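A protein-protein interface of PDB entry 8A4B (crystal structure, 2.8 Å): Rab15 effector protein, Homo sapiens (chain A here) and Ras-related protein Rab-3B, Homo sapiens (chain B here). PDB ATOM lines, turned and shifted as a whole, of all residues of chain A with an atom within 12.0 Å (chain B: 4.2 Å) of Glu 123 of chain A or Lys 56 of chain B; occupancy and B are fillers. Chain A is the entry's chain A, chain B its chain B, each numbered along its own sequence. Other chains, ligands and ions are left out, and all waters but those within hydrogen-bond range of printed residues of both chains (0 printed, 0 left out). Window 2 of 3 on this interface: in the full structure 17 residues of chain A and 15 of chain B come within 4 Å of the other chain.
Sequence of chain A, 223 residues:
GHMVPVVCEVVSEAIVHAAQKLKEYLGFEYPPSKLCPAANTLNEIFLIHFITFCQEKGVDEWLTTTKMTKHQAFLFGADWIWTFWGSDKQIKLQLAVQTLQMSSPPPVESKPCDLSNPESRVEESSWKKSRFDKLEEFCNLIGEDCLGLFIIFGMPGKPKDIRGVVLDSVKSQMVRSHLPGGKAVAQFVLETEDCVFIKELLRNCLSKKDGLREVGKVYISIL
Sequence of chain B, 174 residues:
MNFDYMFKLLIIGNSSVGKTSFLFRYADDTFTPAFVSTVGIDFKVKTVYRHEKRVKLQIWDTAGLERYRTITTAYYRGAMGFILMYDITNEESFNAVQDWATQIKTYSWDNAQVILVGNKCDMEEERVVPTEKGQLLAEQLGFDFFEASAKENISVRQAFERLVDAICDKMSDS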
ATOM      1  N   HIS A  71       2.478 -32.543   8.761  1.00  0.00           N
ATOM      2  CA  HIS A  71       2.111 -31.139   8.888  1.00  0.00           C
ATOM      3  C   HIS A  71       3.342 -30.265   9.095  1.00  0.00           C
ATOM      4  O   HIS A  71       3.490 -29.218   8.453  1.00  0.00           O
ATOM      5  CB  HIS A  71       1.119 -30.968  10.035  1.00  0.00           C
ATOM      6  CG  HIS A  71      -0.226 -31.564   9.759  1.00  0.00           C
ATOM      7  ND1 HIS A  71      -1.263 -31.516  10.665  1.00  0.00           N
ATOM      8  CD2 HIS A  71      -0.706 -32.214   8.673  1.00  0.00           C
ATOM      9  CE1 HIS A  71      -2.324 -32.112  10.150  1.00  0.00           C
ATOM     10  NE2 HIS A  71      -2.012 -32.544   8.941  1.00  0.00           N
ATOM     11  N   PHE A  74       5.383 -30.071   5.869  1.00  0.00           N
ATOM     12  CA  PHE A  74       4.776 -29.160   4.906  1.00  0.00           C
ATOM     13  C   PHE A  74       4.976 -27.704   5.309  1.00  0.00           C
ATOM     14  O   PHE A  74       5.289 -26.859   4.463  1.00  0.00           O
ATOM     15  CB  PHE A  74       3.291 -29.472   4.755  1.00  0.00           C
ATOM     16  CG  PHE A  74       2.551 -28.480   3.911  1.00  0.00           C
ATOM     17  CD1 PHE A  74       2.626 -28.533   2.530  1.00  0.00           C
ATOM     18  CD2 PHE A  74       1.776 -27.495   4.497  1.00  0.00           C
ATOM     19  CE1 PHE A  74       1.945 -27.622   1.751  1.00  0.00           C
ATOM     20  CE2 PHE A  74       1.090 -26.583   3.723  1.00  0.00           C
ATOM     21  CZ  PHE A  74       1.175 -26.646   2.347  1.00  0.00           C
ATOM     22  N   LEU A  75       4.795 -27.388   6.595  1.00  0.00           N
ATOM     23  CA  LEU A  75       4.846 -25.993   7.025  1.00  0.00           C
ATOM     24  C   LEU A  75       6.269 -25.449   7.029  1.00  0.00           C
ATOM     25  O   LEU A  75       6.509 -24.322   6.581  1.00  0.00           O
ATOM     26  CB  LEU A  75       4.235 -25.850   8.416  1.00  0.00           C
ATOM     27  CG  LEU A  75       2.724 -26.004   8.544  1.00  0.00           C
ATOM     28  CD1 LEU A  75       2.339 -26.005  10.010  1.00  0.00           C
ATOM     29  CD2 LEU A  75       2.008 -24.891   7.801  1.00  0.00           C
ATOM     30  N   PRO A 118       2.789 -32.573  -1.636  1.00  0.00           N
ATOM     31  CA  PRO A 118       1.349 -32.789  -1.412  1.00  0.00           C
ATOM     32  C   PRO A 118       0.865 -31.993  -0.206  1.00  0.00           C
ATOM     33  O   PRO A 118       1.489 -32.013   0.859  1.00  0.00           O
ATOM     34  CB  PRO A 118       1.245 -34.302  -1.162  1.00  0.00           C
ATOM     35  CG  PRO A 118       2.608 -34.872  -1.515  1.00  0.00           C
ATOM     36  CD  PRO A 118       3.579 -33.760  -1.274  1.00  0.00           C
ATOM     37  N   GLU A 119      -0.255 -31.295  -0.377  1.00  0.00           N
ATOM     38  CA  GLU A 119      -0.735 -30.399   0.661  1.00  0.00           C
ATOM     39  C   GLU A 119      -1.499 -31.166   1.736  1.00  0.00           C
ATOM     40  O   GLU A 119      -2.000 -32.273   1.518  1.00  0.00           O
ATOM     41  CB  GLU A 119      -1.625 -29.302   0.067  1.00  0.00           C
ATOM     42  CG  GLU A 119      -1.820 -28.095   0.989  1.00  0.00           C
ATOM     43  CD  GLU A 119      -2.790 -27.071   0.434  1.00  0.00           C
ATOM     44  OE1 GLU A 119      -3.524 -27.403  -0.519  1.00  0.00           O
ATOM     45  OE2 GLU A 119      -2.818 -25.931   0.949  1.00  0.00           O
ATOM     46  N   SER A 120      -1.586 -30.552   2.911  1.00  0.00           N
ATOM     47  CA  SER A 120      -2.363 -31.095   4.015  1.00  0.00           C
ATOM     48  C   SER A 120      -3.839 -30.775   3.780  1.00  0.00           C
ATOM     49  O   SER A 120      -4.260 -30.436   2.670  1.00  0.00           O
ATOM     50  CB  SER A 120      -1.847 -30.532   5.335  1.00  0.00           C
ATOM     51  OG  SER A 120      -0.430 -30.395   5.292  1.00  0.00           O
ATOM     52  N   ARG A 121      -4.657 -30.908   4.826  1.00  0.00           N
ATOM     53  CA  ARG A 121      -6.053 -30.493   4.775  1.00  0.00           C
ATOM     54  C   ARG A 121      -6.262 -29.075   5.293  1.00  0.00           C
ATOM     55  O   ARG A 121      -7.324 -28.771   5.854  1.00  0.00           O
ATOM     56  CB  ARG A 121      -6.912 -31.485   5.556  1.00  0.00           C
ATOM     57  CG  ARG A 121      -6.502 -31.620   7.004  1.00  0.00           C
ATOM     58  CD  ARG A 121      -7.191 -32.797   7.660  1.00  0.00           C
ATOM     59  NE  ARG A 121      -6.879 -32.880   9.082  1.00  0.00           N
ATOM     60  CZ  ARG A 121      -5.760 -33.395   9.576  1.00  0.00           C
ATOM     61  NH1 ARG A 121      -4.813 -33.876   8.784  1.00  0.00           N
ATOM     62  NH2 ARG A 121      -5.586 -33.425  10.895  1.00  0.00           N
ATOM     63  N   VAL A 122      -5.267 -28.199   5.128  1.00  0.00           N
ATOM     64  CA  VAL A 122      -5.412 -26.805   5.527  1.00  0.00           C
ATOM     65  C   VAL A 122      -6.405 -26.112   4.604  1.00  0.00           C
ATOM     66  O   VAL A 122      -6.418 -26.343   3.386  1.00  0.00           O
ATOM     67  CB  VAL A 122      -4.048 -26.093   5.508  1.00  0.00           C
ATOM     68  CG1 VAL A 122      -4.105 -24.807   6.321  1.00  0.00           C
ATOM     69  CG2 VAL A 122      -2.948 -27.013   6.020  1.00  0.00           C
ATOM     70  N   GLU A 123      -7.250 -25.245   5.180  1.00  0.00           N
ATOM     71  CA  GLU A 123      -8.313 -24.594   4.419  1.00  0.00           C
ATOM     72  C   GLU A 123      -8.453 -23.113   4.765  1.00  0.00           C
ATOM     73  O   GLU A 123      -9.532 -22.535   4.587  1.00  0.00           O
ATOM     74  CB  GLU A 123      -9.657 -25.300   4.637  1.00  0.00           C
ATOM     75  CG  GLU A 123      -9.993 -26.376   3.610  1.00  0.00           C
ATOM     76  CD  GLU A 123     -11.010 -25.910   2.578  1.00  0.00           C
ATOM     77  OE1 GLU A 123     -11.420 -24.729   2.628  1.00  0.00           O
ATOM     78  OE2 GLU A 123     -11.402 -26.729   1.719  1.00  0.00           O
ATOM     79  N   GLU A 124      -7.389 -22.479   5.248  1.00  0.00           N
ATOM     80  CA  GLU A 124      -7.456 -21.057   5.581  1.00  0.00           C
ATOM     81  C   GLU A 124      -6.768 -20.212   4.512  1.00  0.00           C
ATOM     82  O   GLU A 124      -6.140 -20.741   3.596  1.00  0.00           O
ATOM     83  CB  GLU A 124      -6.829 -20.782   6.952  1.00  0.00           C
ATOM     84  CG  GLU A 124      -5.321 -20.571   6.929  1.00  0.00           C
ATOM     85  CD  GLU A 124      -4.775 -20.105   8.271  1.00  0.00           C
ATOM     86  OE1 GLU A 124      -5.433 -20.349   9.303  1.00  0.00           O
ATOM     87  OE2 GLU A 124      -3.687 -19.489   8.289  1.00  0.00           O
ATOM     88  N   SER A 126      -3.306 -19.622   0.360  1.00  0.00           N
ATOM     89  CA  SER A 126      -2.565 -19.077   1.491  1.00  0.00           C
ATOM     90  C   SER A 126      -1.129 -19.604   1.536  1.00  0.00           C
ATOM     91  O   SER A 126      -0.180 -18.830   1.675  1.00  0.00           O
ATOM     92  CB  SER A 126      -3.283 -19.403   2.803  1.00  0.00           C
ATOM     93  OG  SER A 126      -2.541 -18.940   3.917  1.00  0.00           O
ATOM     94  N   TRP A 127      -0.978 -20.920   1.411  1.00  0.00           N
ATOM     95  CA  TRP A 127       0.317 -21.595   1.515  1.00  0.00           C
ATOM     96  C   TRP A 127       0.639 -22.192   0.148  1.00  0.00           C
ATOM     97  O   TRP A 127       0.385 -23.370  -0.107  1.00  0.00           O
ATOM     98  CB  TRP A 127       0.300 -22.688   2.599  1.00  0.00           C
ATOM     99  CG  TRP A 127      -0.723 -22.489   3.684  1.00  0.00           C
ATOM    100  CD1 TRP A 127      -2.082 -22.588   3.564  1.00  0.00           C
ATOM    101  CD2 TRP A 127      -0.465 -22.191   5.059  1.00  0.00           C
ATOM    102  NE1 TRP A 127      -2.684 -22.345   4.772  1.00  0.00           N
ATOM    103  CE2 TRP A 127      -1.714 -22.104   5.709  1.00  0.00           C
ATOM    104  CE3 TRP A 127       0.698 -21.979   5.804  1.00  0.00           C
ATOM    105  CZ2 TRP A 127      -1.830 -21.815   7.066  1.00  0.00           C
ATOM    106  CZ3 TRP A 127       0.581 -21.693   7.151  1.00  0.00           C
ATOM    107  CH2 TRP A 127      -0.674 -21.615   7.769  1.00  0.00           C
ATOM    108  N   LYS A 128       1.221 -21.375  -0.730  1.00  0.00           N
ATOM    109  CA  LYS A 128       1.580 -21.818  -2.072  1.00  0.00           C
ATOM    110  C   LYS A 128       3.063 -21.624  -2.363  1.00  0.00           C
ATOM    111  O   LYS A 128       3.458 -21.533  -3.531  1.00  0.00           O
ATOM    112  CB  LYS A 128       0.728 -21.096  -3.115  1.00  0.00           C
ATOM    113  CG  LYS A 128      -0.325 -21.976  -3.770  1.00  0.00           C
ATOM    114  CD  LYS A 128      -1.246 -22.611  -2.740  1.00  0.00           C
ATOM    115  CE  LYS A 128      -2.075 -21.566  -2.008  1.00  0.00           C
ATOM    116  NZ  LYS A 128      -3.025 -22.200  -1.053  1.00  0.00           N
ATOM    117  N   PHE B   3     -18.277 -28.673   5.588  1.00  0.00           N
ATOM    118  CA  PHE B   3     -18.553 -28.094   6.896  1.00  0.00           C
ATOM    119  C   PHE B   3     -19.274 -26.767   6.708  1.00  0.00           C
ATOM    120  O   PHE B   3     -19.435 -26.276   5.588  1.00  0.00           O
ATOM    121  CB  PHE B   3     -17.261 -27.910   7.698  1.00  0.00           C
ATOM    122  CG  PHE B   3     -16.130 -27.334   6.893  1.00  0.00           C
ATOM    123  CD1 PHE B   3     -15.979 -25.960   6.767  1.00  0.00           C
ATOM    124  CD2 PHE B   3     -15.224 -28.164   6.252  1.00  0.00           C
ATOM    125  CE1 PHE B   3     -14.939 -25.427   6.020  1.00  0.00           C
ATOM    126  CE2 PHE B   3     -14.184 -27.637   5.503  1.00  0.00           C
ATOM    127  CZ  PHE B   3     -14.042 -26.267   5.387  1.00  0.00           C
ATOM    128  N   TYR B   5     -18.668 -24.074   9.371  1.00  0.00           N
ATOM    129  CA  TYR B   5     -17.755 -23.064   9.893  1.00  0.00           C
ATOM    130  C   TYR B   5     -16.371 -23.675  10.065  1.00  0.00           C
ATOM    131  O   TYR B   5     -16.227 -24.888  10.214  1.00  0.00           O
ATOM    132  CB  TYR B   5     -18.238 -22.487  11.232  1.00  0.00           C
ATOM    133  CG  TYR B   5     -19.398 -21.522  11.125  1.00  0.00           C
ATOM    134  CD1 TYR B   5     -19.205 -20.223  10.673  1.00  0.00           C
ATOM    135  CD2 TYR B   5     -20.682 -21.904  11.496  1.00  0.00           C
ATOM    136  CE1 TYR B   5     -20.260 -19.333  10.580  1.00  0.00           C
ATOM    137  CE2 TYR B   5     -21.744 -21.022  11.407  1.00  0.00           C
ATOM    138  CZ  TYR B   5     -21.528 -19.738  10.949  1.00  0.00           C
ATOM    139  OH  TYR B   5     -22.583 -18.858  10.859  1.00  0.00           O
ATOM    140  N   MET B   6     -15.346 -22.823  10.043  1.00  0.00           N
ATOM    141  CA  MET B   6     -13.990 -23.244  10.377  1.00  0.00           C
ATOM    142  C   MET B   6     -13.347 -22.197  11.269  1.00  0.00           C
ATOM    143  O   MET B   6     -13.283 -21.020  10.900  1.00  0.00           O
ATOM    144  CB  MET B   6     -13.126 -23.458   9.131  1.00  0.00           C
ATOM    145  CG  MET B   6     -11.754 -24.036   9.460  1.00  0.00           C
ATOM    146  SD  MET B   6     -10.566 -24.009   8.101  1.00  0.00           S
ATOM    147  CE  MET B   6      -9.619 -22.543   8.516  1.00  0.00           C
ATOM    148  N   PHE B   7     -12.862 -22.622  12.432  1.00  0.00           N
ATOM    149  CA  PHE B   7     -12.277 -21.720  13.414  1.00  0.00           C
ATOM    150  C   PHE B   7     -10.821 -22.094  13.647  1.00  0.00           C
ATOM    151  O   PHE B   7     -10.501 -23.272  13.857  1.00  0.00           O
ATOM    152  CB  PHE B   7     -13.046 -21.758  14.742  1.00  0.00           C
ATOM    153  CG  PHE B   7     -14.469 -21.274  14.640  1.00  0.00           C
ATOM    154  CD1 PHE B   7     -14.874 -20.461  13.596  1.00  0.00           C
ATOM    155  CD2 PHE B   7     -15.404 -21.636  15.598  1.00  0.00           C
ATOM    156  CE1 PHE B   7     -16.182 -20.021  13.504  1.00  0.00           C
ATOM    157  CE2 PHE B   7     -16.715 -21.200  15.515  1.00  0.00           C
ATOM    158  CZ  PHE B   7     -17.103 -20.391  14.466  1.00  0.00           C
ATOM    159  N   VAL B  45      -6.835 -31.251  13.373  1.00  0.00           N
ATOM    160  CA  VAL B  45      -8.162 -30.836  12.941  1.00  0.00           C
ATOM    161  C   VAL B  45      -9.188 -31.705  13.648  1.00  0.00           C
ATOM    162  O   VAL B  45      -9.053 -32.935  13.674  1.00  0.00           O
ATOM    163  CB  VAL B  45      -8.312 -30.935  11.412  1.00  0.00           C
ATOM    164  CG1 VAL B  45      -9.717 -30.558  11.002  1.00  0.00           C
ATOM    165  CG2 VAL B  45      -7.291 -30.037  10.717  1.00  0.00           C
ATOM    166  N   LYS B  46     -10.195 -31.070  14.243  1.00  0.00           N
ATOM    167  CA  LYS B  46     -11.285 -31.794  14.889  1.00  0.00           C
ATOM    168  C   LYS B  46     -12.619 -31.201  14.462  1.00  0.00           C
ATOM    169  O   LYS B  46     -12.785 -29.980  14.457  1.00  0.00           O
ATOM    170  CB  LYS B  46     -11.164 -31.764  16.418  1.00  0.00           C
ATOM    171  CG  LYS B  46     -12.224 -32.612  17.124  1.00  0.00           C
ATOM    172  CD  LYS B  46     -12.134 -32.501  18.637  1.00  0.00           C
ATOM    173  CE  LYS B  46     -13.223 -33.314  19.326  1.00  0.00           C
ATOM    174  NZ  LYS B  46     -12.993 -34.788  19.244  1.00  0.00           N
ATOM    175  N   ARG B  54     -22.166 -27.634  11.796  1.00  0.00           N
ATOM    176  CA  ARG B  54     -20.900 -28.346  11.686  1.00  0.00           C
ATOM    177  C   ARG B  54     -19.758 -27.337  11.725  1.00  0.00           C
ATOM    178  O   ARG B  54     -19.635 -26.487  10.829  1.00  0.00           O
ATOM    179  CB  ARG B  54     -20.851 -29.175  10.403  1.00  0.00           C
ATOM    180  CG  ARG B  54     -21.972 -30.205  10.292  1.00  0.00           C
ATOM    181  CD  ARG B  54     -21.922 -30.974   8.973  1.00  0.00           C
ATOM    182  NE  ARG B  54     -21.047 -32.140   9.032  1.00  0.00           N
ATOM    183  CZ  ARG B  54     -19.755 -32.127   8.734  1.00  0.00           C
ATOM    184  NH1 ARG B  54     -19.142 -31.014   8.365  1.00  0.00           N
ATOM    185  NH2 ARG B  54     -19.061 -33.259   8.808  1.00  0.00           N
ATOM    186  N   VAL B  55     -18.933 -27.421  12.767  1.00  0.00           N
ATOM    187  CA  VAL B  55     -17.823 -26.503  12.969  1.00  0.00           C
ATOM    188  C   VAL B  55     -16.535 -27.315  12.966  1.00  0.00           C
ATOM    189  O   VAL B  55     -16.362 -28.222  13.790  1.00  0.00           O
ATOM    190  CB  VAL B  55     -17.972 -25.710  14.277  1.00  0.00           C
ATOM    191  CG1 VAL B  55     -16.830 -24.719  14.435  1.00  0.00           C
ATOM    192  CG2 VAL B  55     -19.315 -24.990  14.315  1.00  0.00           C
ATOM    193  N   LYS B  56     -15.639 -26.994  12.040  1.00  0.00           N
ATOM    194  CA  LYS B  56     -14.300 -27.554  12.022  1.00  0.00           C
ATOM    195  C   LYS B  56     -13.378 -26.664  12.845  1.00  0.00           C
ATOM    196  O   LYS B  56     -13.490 -25.435  12.818  1.00  0.00           O
ATOM    197  CB  LYS B  56     -13.784 -27.672  10.588  1.00  0.00           C
ATOM    198  CG  LYS B  56     -12.707 -28.719  10.409  1.00  0.00           C
ATOM    199  CD  LYS B  56     -12.150 -28.706   8.995  1.00  0.00           C
ATOM    200  CE  LYS B  56     -11.314 -27.462   8.750  1.00  0.00           C
ATOM    201  NZ  LYS B  56     -10.748 -27.415   7.372  1.00  0.00           N
ATOM    202  N   LEU B  57     -12.484 -27.293  13.600  1.00  0.00           N
ATOM    203  CA  LEU B  57     -11.543 -26.602  14.465  1.00  0.00           C
ATOM    204  C   LEU B  57     -10.143 -26.966  14.006  1.00  0.00           C
ATOM    205  O   LEU B  57      -9.771 -28.147  14.017  1.00  0.00           O
ATOM    206  CB  LEU B  57     -11.747 -26.996  15.930  1.00  0.00           C
ATOM    207  CG  LEU B  57     -13.152 -26.861  16.509  1.00  0.00           C
ATOM    208  CD1 LEU B  57     -13.178 -27.365  17.939  1.00  0.00           C
ATOM    209  CD2 LEU B  57     -13.625 -25.424  16.441  1.00  0.00           C
ATOM    210  N   GLN B  58      -9.380 -25.960  13.590  1.00  0.00           N
ATOM    211  CA  GLN B  58      -7.975 -26.135  13.248  1.00  0.00           C
ATOM    212  C   GLN B  58      -7.193 -25.658  14.463  1.00  0.00           C
ATOM    213  O   GLN B  58      -7.049 -24.451  14.689  1.00  0.00           O
ATOM    214  CB  GLN B  58      -7.618 -25.360  11.984  1.00  0.00           C
ATOM    215  CG  GLN B  58      -6.338 -25.820  11.316  1.00  0.00           C
ATOM    216  CD  GLN B  58      -5.999 -24.994  10.092  1.00  0.00           C
ATOM    217  OE1 GLN B  58      -5.631 -25.534   9.048  1.00  0.00           O
ATOM    218  NE2 GLN B  58      -6.118 -23.674  10.214  1.00  0.00           N
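Printed residues of chain B that touch a printed residue of chain A: Met 6, Val 45, Lys 56 and Gln 58.
Hydrophobic or aromatic side chains of chain B that line the printed part of chain A: Met 6 and Val 45.
Among the printed residues, 7 pairs touch across the chains.
SD of Met 6 of chain B lies within hydrogen-bond range of NZ of Lys 56 of chain B, 3.5 Å away.
The backbone carbonyl oxygen (O) of Lys 56 of chain B is in hydrogen-bond range of the backbone NH (N) of Phe 7 of chain B (2.9 Å).
O of Phe 7 of chain B lies within hydrogen-bond range of N of Gln 58 of chain B, at 2.9 Å.
NE2 of His 71 of chain A sits at hydrogen-bond distance from NH1 of Arg 121 of chain A (3.1 Å).
The backbone NH (N) of Lys 56 of chain B is in hydrogen-bond range of the backbone carbonyl oxygen (O) of Tyr 5 of chain B (2.8 Å).
Of chain B, only Met 6 and Lys 56 come within 4 Å of Glu 123 of chain A.
Phe 3 of chain B touches none of the printed residues of chain A.
Met 6 of chain B touches just these residues of chain A: Glu 123 (3.8 Å) and Glu 124 (3.7 Å).
No residue of chain A comes within 4 Å of Phe 7 of chain B.
Of chain A, only Arg 121 (3.3 Å) comes within 4 Å of Val 45 of chain B.
No residue of chain A comes within 4 Å of Val 55 of chain B.
No residue of chain A comes within 4 Å of Leu 57 of chain B.
Printed residues of chain B within 4 Å of Arg 121 of chain A: Val 45 and Lys 56.
Printed residues of chain B within 4 Å of Val 122 of chain A: Gln 58 (3.2 Å).
Printed residues of chain B within 4 Å of Glu 124 of chain A: Met 6 and Gln 58.
His 71 of chain A touches none of the printed residues of chain B.
Lys 128 of chain A touches none of the printed residues of chain B.
The nearest residue of chain B that does not touch Glu 123 of chain A is Phe 3 of chain B (4.1 Å).
The nearest printed residue of chain B that does not touch Arg 121 of chain A is Gln 58 of chain B (4.9 Å).
Among the printed residues, pairs that only touch across the chains: Arg 121 of chain A with Val 45 of chain B (3.3 Å), Arg 121 of chain A with Lys 56 of chain B (3.98 Å), Val 122 of chain A with Gln 58 of chain B (3.2 Å), Glu 123 of chain A with Met 6 of chain B (3.8 Å), Glu 123 of chain A with Lys 56 of chain B (3.6 Å), Glu 124 of chain A with Met 6 of chain B (3.7 Å) and Glu 124 of chain A with Gln 58 of chain B (3.5 Å).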
